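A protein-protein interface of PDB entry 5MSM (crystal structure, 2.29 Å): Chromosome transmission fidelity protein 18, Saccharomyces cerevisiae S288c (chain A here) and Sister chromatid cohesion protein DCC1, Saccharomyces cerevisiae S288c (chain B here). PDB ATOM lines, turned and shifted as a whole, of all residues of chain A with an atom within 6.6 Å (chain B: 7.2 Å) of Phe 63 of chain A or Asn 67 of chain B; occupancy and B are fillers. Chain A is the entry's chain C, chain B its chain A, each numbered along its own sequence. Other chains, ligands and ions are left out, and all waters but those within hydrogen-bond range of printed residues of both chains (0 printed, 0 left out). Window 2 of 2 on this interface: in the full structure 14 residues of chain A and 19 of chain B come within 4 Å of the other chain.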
ATOM      1  N   ASN A  60     -30.205   6.677   5.093  1.00  0.00           N
ATOM      2  CA  ASN A  60     -29.466   7.842   4.606  1.00  0.00           C
ATOM      3  C   ASN A  60     -30.351   8.550   3.619  1.00  0.00           C
ATOM      4  O   ASN A  60     -30.983   7.893   2.790  1.00  0.00           O
ATOM      5  CB  ASN A  60     -28.150   7.445   3.944  1.00  0.00           C
ATOM      6  CG  ASN A  60     -27.171   6.844   4.910  1.00  0.00           C
ATOM      7  OD1 ASN A  60     -27.175   7.154   6.101  1.00  0.00           O
ATOM      8  ND2 ASN A  60     -26.330   5.944   4.405  1.00  0.00           N
ATOM      9  N   GLU A  61     -30.397   9.878   3.699  1.00  0.00           N
ATOM     10  CA  GLU A  61     -31.318  10.637   2.876  1.00  0.00           C
ATOM     11  C   GLU A  61     -30.936  10.545   1.409  1.00  0.00           C
ATOM     12  O   GLU A  61     -31.780  10.616   0.526  1.00  0.00           O
ATOM     13  CB  GLU A  61     -31.370  12.096   3.330  1.00  0.00           C
ATOM     14  CG  GLU A  61     -31.939  12.270   4.716  1.00  0.00           C
ATOM     15  CD  GLU A  61     -33.366  11.715   4.832  1.00  0.00           C
ATOM     16  OE1 GLU A  61     -33.720  11.207   5.925  1.00  0.00           O
ATOM     17  OE2 GLU A  61     -34.127  11.784   3.835  1.00  0.00           O
ATOM     18  N   GLY A  62     -29.645  10.419   1.146  1.00  0.00           N
ATOM     19  CA  GLY A  62     -29.196  10.137  -0.198  1.00  0.00           C
ATOM     20  C   GLY A  62     -27.896   9.364  -0.219  1.00  0.00           C
ATOM     21  O   GLY A  62     -27.634   8.562   0.668  1.00  0.00           O
ATOM     22  N   PHE A  63     -27.097   9.595  -1.254  1.00  0.00           N
ATOM     23  CA  PHE A  63     -25.960   8.734  -1.569  1.00  0.00           C
ATOM     24  C   PHE A  63     -24.736   9.568  -1.985  1.00  0.00           C
ATOM     25  O   PHE A  63     -24.836  10.449  -2.846  1.00  0.00           O
ATOM     26  CB  PHE A  63     -26.337   7.717  -2.678  1.00  0.00           C
ATOM     27  CG  PHE A  63     -25.168   6.882  -3.176  1.00  0.00           C
ATOM     28  CD1 PHE A  63     -24.659   5.834  -2.404  1.00  0.00           C
ATOM     29  CD2 PHE A  63     -24.581   7.138  -4.419  1.00  0.00           C
ATOM     30  CE1 PHE A  63     -23.582   5.046  -2.863  1.00  0.00           C
ATOM     31  CE2 PHE A  63     -23.503   6.374  -4.870  1.00  0.00           C
ATOM     32  CZ  PHE A  63     -23.000   5.328  -4.082  1.00  0.00           C
ATOM     33  N   SER A  64     -23.594   9.267  -1.365  1.00  0.00           N
ATOM     34  CA  SER A  64     -22.310   9.893  -1.672  1.00  0.00           C
ATOM     35  C   SER A  64     -21.328   8.838  -2.131  1.00  0.00           C
ATOM     36  O   SER A  64     -21.114   7.826  -1.452  1.00  0.00           O
ATOM     37  CB  SER A  64     -21.714  10.588  -0.455  1.00  0.00           C
ATOM     38  OG  SER A  64     -22.359  11.809  -0.145  1.00  0.00           O
ATOM     39  N   ASN A  65     -20.744   9.114  -3.289  1.00  0.00           N
ATOM     40  CA  ASN A  65     -19.683   8.368  -3.936  1.00  0.00           C
ATOM     41  C   ASN A  65     -18.488   9.296  -3.810  1.00  0.00           C
ATOM     42  O   ASN A  65     -18.563  10.433  -4.260  1.00  0.00           O
ATOM     43  CB  ASN A  65     -20.031   8.117  -5.410  1.00  0.00           C
ATOM     44  CG  ASN A  65     -19.875   6.671  -5.853  1.00  0.00           C
ATOM     45  OD1 ASN A  65     -19.166   5.871  -5.243  1.00  0.00           O
ATOM     46  ND2 ASN A  65     -20.494   6.351  -6.980  1.00  0.00           N
ATOM     47  N   LYS B  64     -14.573   4.941  -2.333  1.00  0.00           N
ATOM     48  CA  LYS B  64     -15.483   4.754  -1.214  1.00  0.00           C
ATOM     49  C   LYS B  64     -16.886   5.271  -1.544  1.00  0.00           C
ATOM     50  O   LYS B  64     -17.036   6.207  -2.338  1.00  0.00           O
ATOM     51  CB  LYS B  64     -14.930   5.468   0.025  1.00  0.00           C
ATOM     52  CG  LYS B  64     -13.658   4.827   0.538  1.00  0.00           C
ATOM     53  CD  LYS B  64     -13.088   5.553   1.751  1.00  0.00           C
ATOM     54  CE  LYS B  64     -11.764   4.908   2.170  1.00  0.00           C
ATOM     55  NZ  LYS B  64     -11.145   5.595   3.344  1.00  0.00           N
ATOM     56  N   HIS B  65     -17.903   4.658  -0.934  1.00  0.00           N
ATOM     57  CA  HIS B  65     -19.304   5.099  -1.059  1.00  0.00           C
ATOM     58  C   HIS B  65     -19.986   5.056   0.304  1.00  0.00           C
ATOM     59  O   HIS B  65     -19.400   4.576   1.278  1.00  0.00           O
ATOM     60  CB  HIS B  65     -20.065   4.244  -2.058  1.00  0.00           C
ATOM     61  CG  HIS B  65     -20.084   2.797  -1.699  1.00  0.00           C
ATOM     62  ND1 HIS B  65     -20.871   2.292  -0.686  1.00  0.00           N
ATOM     63  CD2 HIS B  65     -19.420   1.740  -2.227  1.00  0.00           C
ATOM     64  CE1 HIS B  65     -20.672   0.988  -0.588  1.00  0.00           C
ATOM     65  NE2 HIS B  65     -19.795   0.628  -1.512  1.00  0.00           N
ATOM     66  N   SER B  66     -21.212   5.574   0.381  1.00  0.00           N
ATOM     67  CA  SER B  66     -21.887   5.778   1.669  1.00  0.00           C
ATOM     68  C   SER B  66     -22.950   4.720   2.074  1.00  0.00           C
ATOM     69  O   SER B  66     -23.456   4.754   3.203  1.00  0.00           O
ATOM     70  CB  SER B  66     -22.537   7.156   1.670  1.00  0.00           C
ATOM     71  OG  SER B  66     -23.466   7.288   0.596  1.00  0.00           O
ATOM     72  N   ASN B  67     -23.255   3.775   1.188  1.00  0.00           N
ATOM     73  CA  ASN B  67     -24.244   2.752   1.491  1.00  0.00           C
ATOM     74  C   ASN B  67     -23.669   1.570   2.231  1.00  0.00           C
ATOM     75  O   ASN B  67     -22.458   1.428   2.352  1.00  0.00           O
ATOM     76  CB  ASN B  67     -24.930   2.269   0.210  1.00  0.00           C
ATOM     77  CG  ASN B  67     -25.875   3.311  -0.364  1.00  0.00           C
ATOM     78  OD1 ASN B  67     -26.233   4.271   0.315  1.00  0.00           O
ATOM     79  ND2 ASN B  67     -26.262   3.141  -1.614  1.00  0.00           N
ATOM     80  N   THR B  68     -24.561   0.723   2.732  1.00  0.00           N
ATOM     81  CA  THR B  68     -24.184  -0.572   3.264  1.00  0.00           C
ATOM     82  C   THR B  68     -24.130  -1.602   2.115  1.00  0.00           C
ATOM     83  O   THR B  68     -25.048  -1.678   1.283  1.00  0.00           O
ATOM     84  CB  THR B  68     -25.175  -1.051   4.330  1.00  0.00           C
ATOM     85  OG1 THR B  68     -25.196  -0.136   5.419  1.00  0.00           O
ATOM     86  CG2 THR B  68     -24.796  -2.418   4.838  1.00  0.00           C
ATOM     87  N   VAL B  69     -23.028  -2.330   1.990  1.00  0.00           N
ATOM     88  CA  VAL B  69     -23.034  -3.458   1.068  1.00  0.00           C
ATOM     89  C   VAL B  69     -22.574  -4.685   1.819  1.00  0.00           C
ATOM     90  O   VAL B  69     -21.430  -4.745   2.291  1.00  0.00           O
ATOM     91  CB  VAL B  69     -22.163  -3.242  -0.149  1.00  0.00           C
ATOM     92  CG1 VAL B  69     -22.172  -4.514  -1.029  1.00  0.00           C
ATOM     93  CG2 VAL B  69     -22.664  -2.055  -0.929  1.00  0.00           C
ATOM     94  N   LEU B  70     -23.486  -5.640   1.971  1.00  0.00           N
ATOM     95  CA  LEU B  70     -23.165  -6.924   2.554  1.00  0.00           C
ATOM     96  C   LEU B  70     -23.044  -7.981   1.488  1.00  0.00           C
ATOM     97  O   LEU B  70     -23.906  -8.089   0.606  1.00  0.00           O
ATOM     98  CB  LEU B  70     -24.225  -7.362   3.550  1.00  0.00           C
ATOM     99  CG  LEU B  70     -24.319  -6.516   4.807  1.00  0.00           C
ATOM    100  CD1 LEU B  70     -25.466  -7.073   5.650  1.00  0.00           C
ATOM    101  CD2 LEU B  70     -22.994  -6.513   5.561  1.00  0.00           C
ATOM    102  N   LYS B 103     -18.572  -6.836   4.588  1.00  0.00           N
ATOM    103  CA  LYS B 103     -19.245  -5.570   4.417  1.00  0.00           C
ATOM    104  C   LYS B 103     -18.287  -4.588   3.775  1.00  0.00           C
ATOM    105  O   LYS B 103     -17.312  -4.185   4.411  1.00  0.00           O
ATOM    106  CB  LYS B 103     -19.708  -5.038   5.751  1.00  0.00           C
ATOM    107  CG  LYS B 103     -20.343  -3.658   5.710  1.00  0.00           C
ATOM    108  CD  LYS B 103     -20.793  -3.276   7.119  1.00  0.00           C
ATOM    109  CE  LYS B 103     -21.264  -1.853   7.155  1.00  0.00           C
ATOM    110  NZ  LYS B 103     -20.184  -0.911   6.701  1.00  0.00           N
ATOM    111  N   THR B 104     -18.557  -4.193   2.533  1.00  0.00           N
ATOM    112  CA  THR B 104     -17.619  -3.364   1.779  1.00  0.00           C
ATOM    113  C   THR B 104     -18.141  -1.931   1.673  1.00  0.00           C
ATOM    114  O   THR B 104     -19.327  -1.723   1.400  1.00  0.00           O
ATOM    115  CB  THR B 104     -17.411  -3.941   0.374  1.00  0.00           C
ATOM    116  OG1 THR B 104     -18.663  -3.911  -0.331  1.00  0.00           O
ATOM    117  CG2 THR B 104     -16.933  -5.372   0.471  1.00  0.00           C
ATOM    118  N   GLU B 105     -17.256  -0.956   1.872  1.00  0.00           N
ATOM    119  CA  GLU B 105     -17.594   0.471   1.800  1.00  0.00           C
ATOM    120  C   GLU B 105     -16.944   1.160   0.599  1.00  0.00           C
ATOM    121  O   GLU B 105     -16.922   2.393   0.528  1.00  0.00           O
ATOM    122  CB  GLU B 105     -17.167   1.170   3.087  1.00  0.00           C
ATOM    123  CG  GLU B 105     -17.442   0.356   4.360  1.00  0.00           C
ATOM    124  CD  GLU B 105     -16.934   1.024   5.646  1.00  0.00           C
ATOM    125  OE1 GLU B 105     -15.853   1.669   5.631  1.00  0.00           O
ATOM    126  OE2 GLU B 105     -17.620   0.897   6.679  1.00  0.00           O
ATOM    127  N   SER B 106     -16.439   0.353  -0.344  1.00  0.00           N
ATOM    128  CA  SER B 106     -15.759   0.846  -1.541  1.00  0.00           C
ATOM    129  C   SER B 106     -15.670  -0.234  -2.604  1.00  0.00           C
ATOM    130  O   SER B 106     -15.828  -1.409  -2.290  1.00  0.00           O
ATOM    131  CB  SER B 106     -14.340   1.315  -1.218  1.00  0.00           C
ATOM    132  OG  SER B 106     -13.537   0.192  -0.909  1.00  0.00           O
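The backbone NH of Ser 64 of chain A sits at hydrogen-bond distance from the side-chain hydroxyl of Ser 66 of chain B (2.8 Å).
The backbone carbonyl oxygen of Ser 66 of chain B lies within hydrogen-bond range of the side-chain amide nitrogen of Asn 60 of chain A, 3.3 Å away.
A ring nitrogen (ND1) of His 65 of chain B lies within hydrogen-bond range of the backbone NH (N) of Asn 67 of chain B, 3.4 Å away.
The backbone NH (N) of His 65 of chain B sits at hydrogen-bond distance from the backbone carbonyl oxygen (O) of Glu 105 of chain B (2.9 Å).
CE1 of Phe 63 of chain A touches CB of His 65 of chain B (3.7 Å).
OG of Ser 66 of chain B touches CD1 of Phe 63 of chain A, 3.5 Å away.
Phe 63 of chain A touches Asn 67 of chain B.
Ser 64 of chain A touches His 65 of chain B (O to CA, 3.3 Å).
Asn 65 of chain A touches Lys 64 of chain B.
Asn 65 of chain A touches His 65 of chain B.
Printed residues of chain B within 4 Å of Asn 60 of chain A: Ser 66.
Of the printed residues of chain B, Asn 65 of chain A touches Lys 64 (3.6 Å) and His 65 (3.7 Å).
Of the printed residues of chain A, Lys 64 of chain B touches Asn 65 (3.6 Å).
The nearest residue of chain B that does not touch Phe 63 of chain A is Lys 64 of chain B (6.3 Å).
The nearest residue of chain A that does not touch Asn 67 of chain B is Asn 60 of chain A (4.4 Å).
Of the 11 printed residues of chain B, 4 touch a printed residue of chain A.
Hydrophobic or aromatic side chains of chain B within 4 Å of the printed part of chain A: His 65.
Along chain B the printed residues that touch a printed residue of chain A span positions 64 to 67.
Hydrophobic or aromatic side chains of chain A that line the printed part of chain B: Phe 63.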
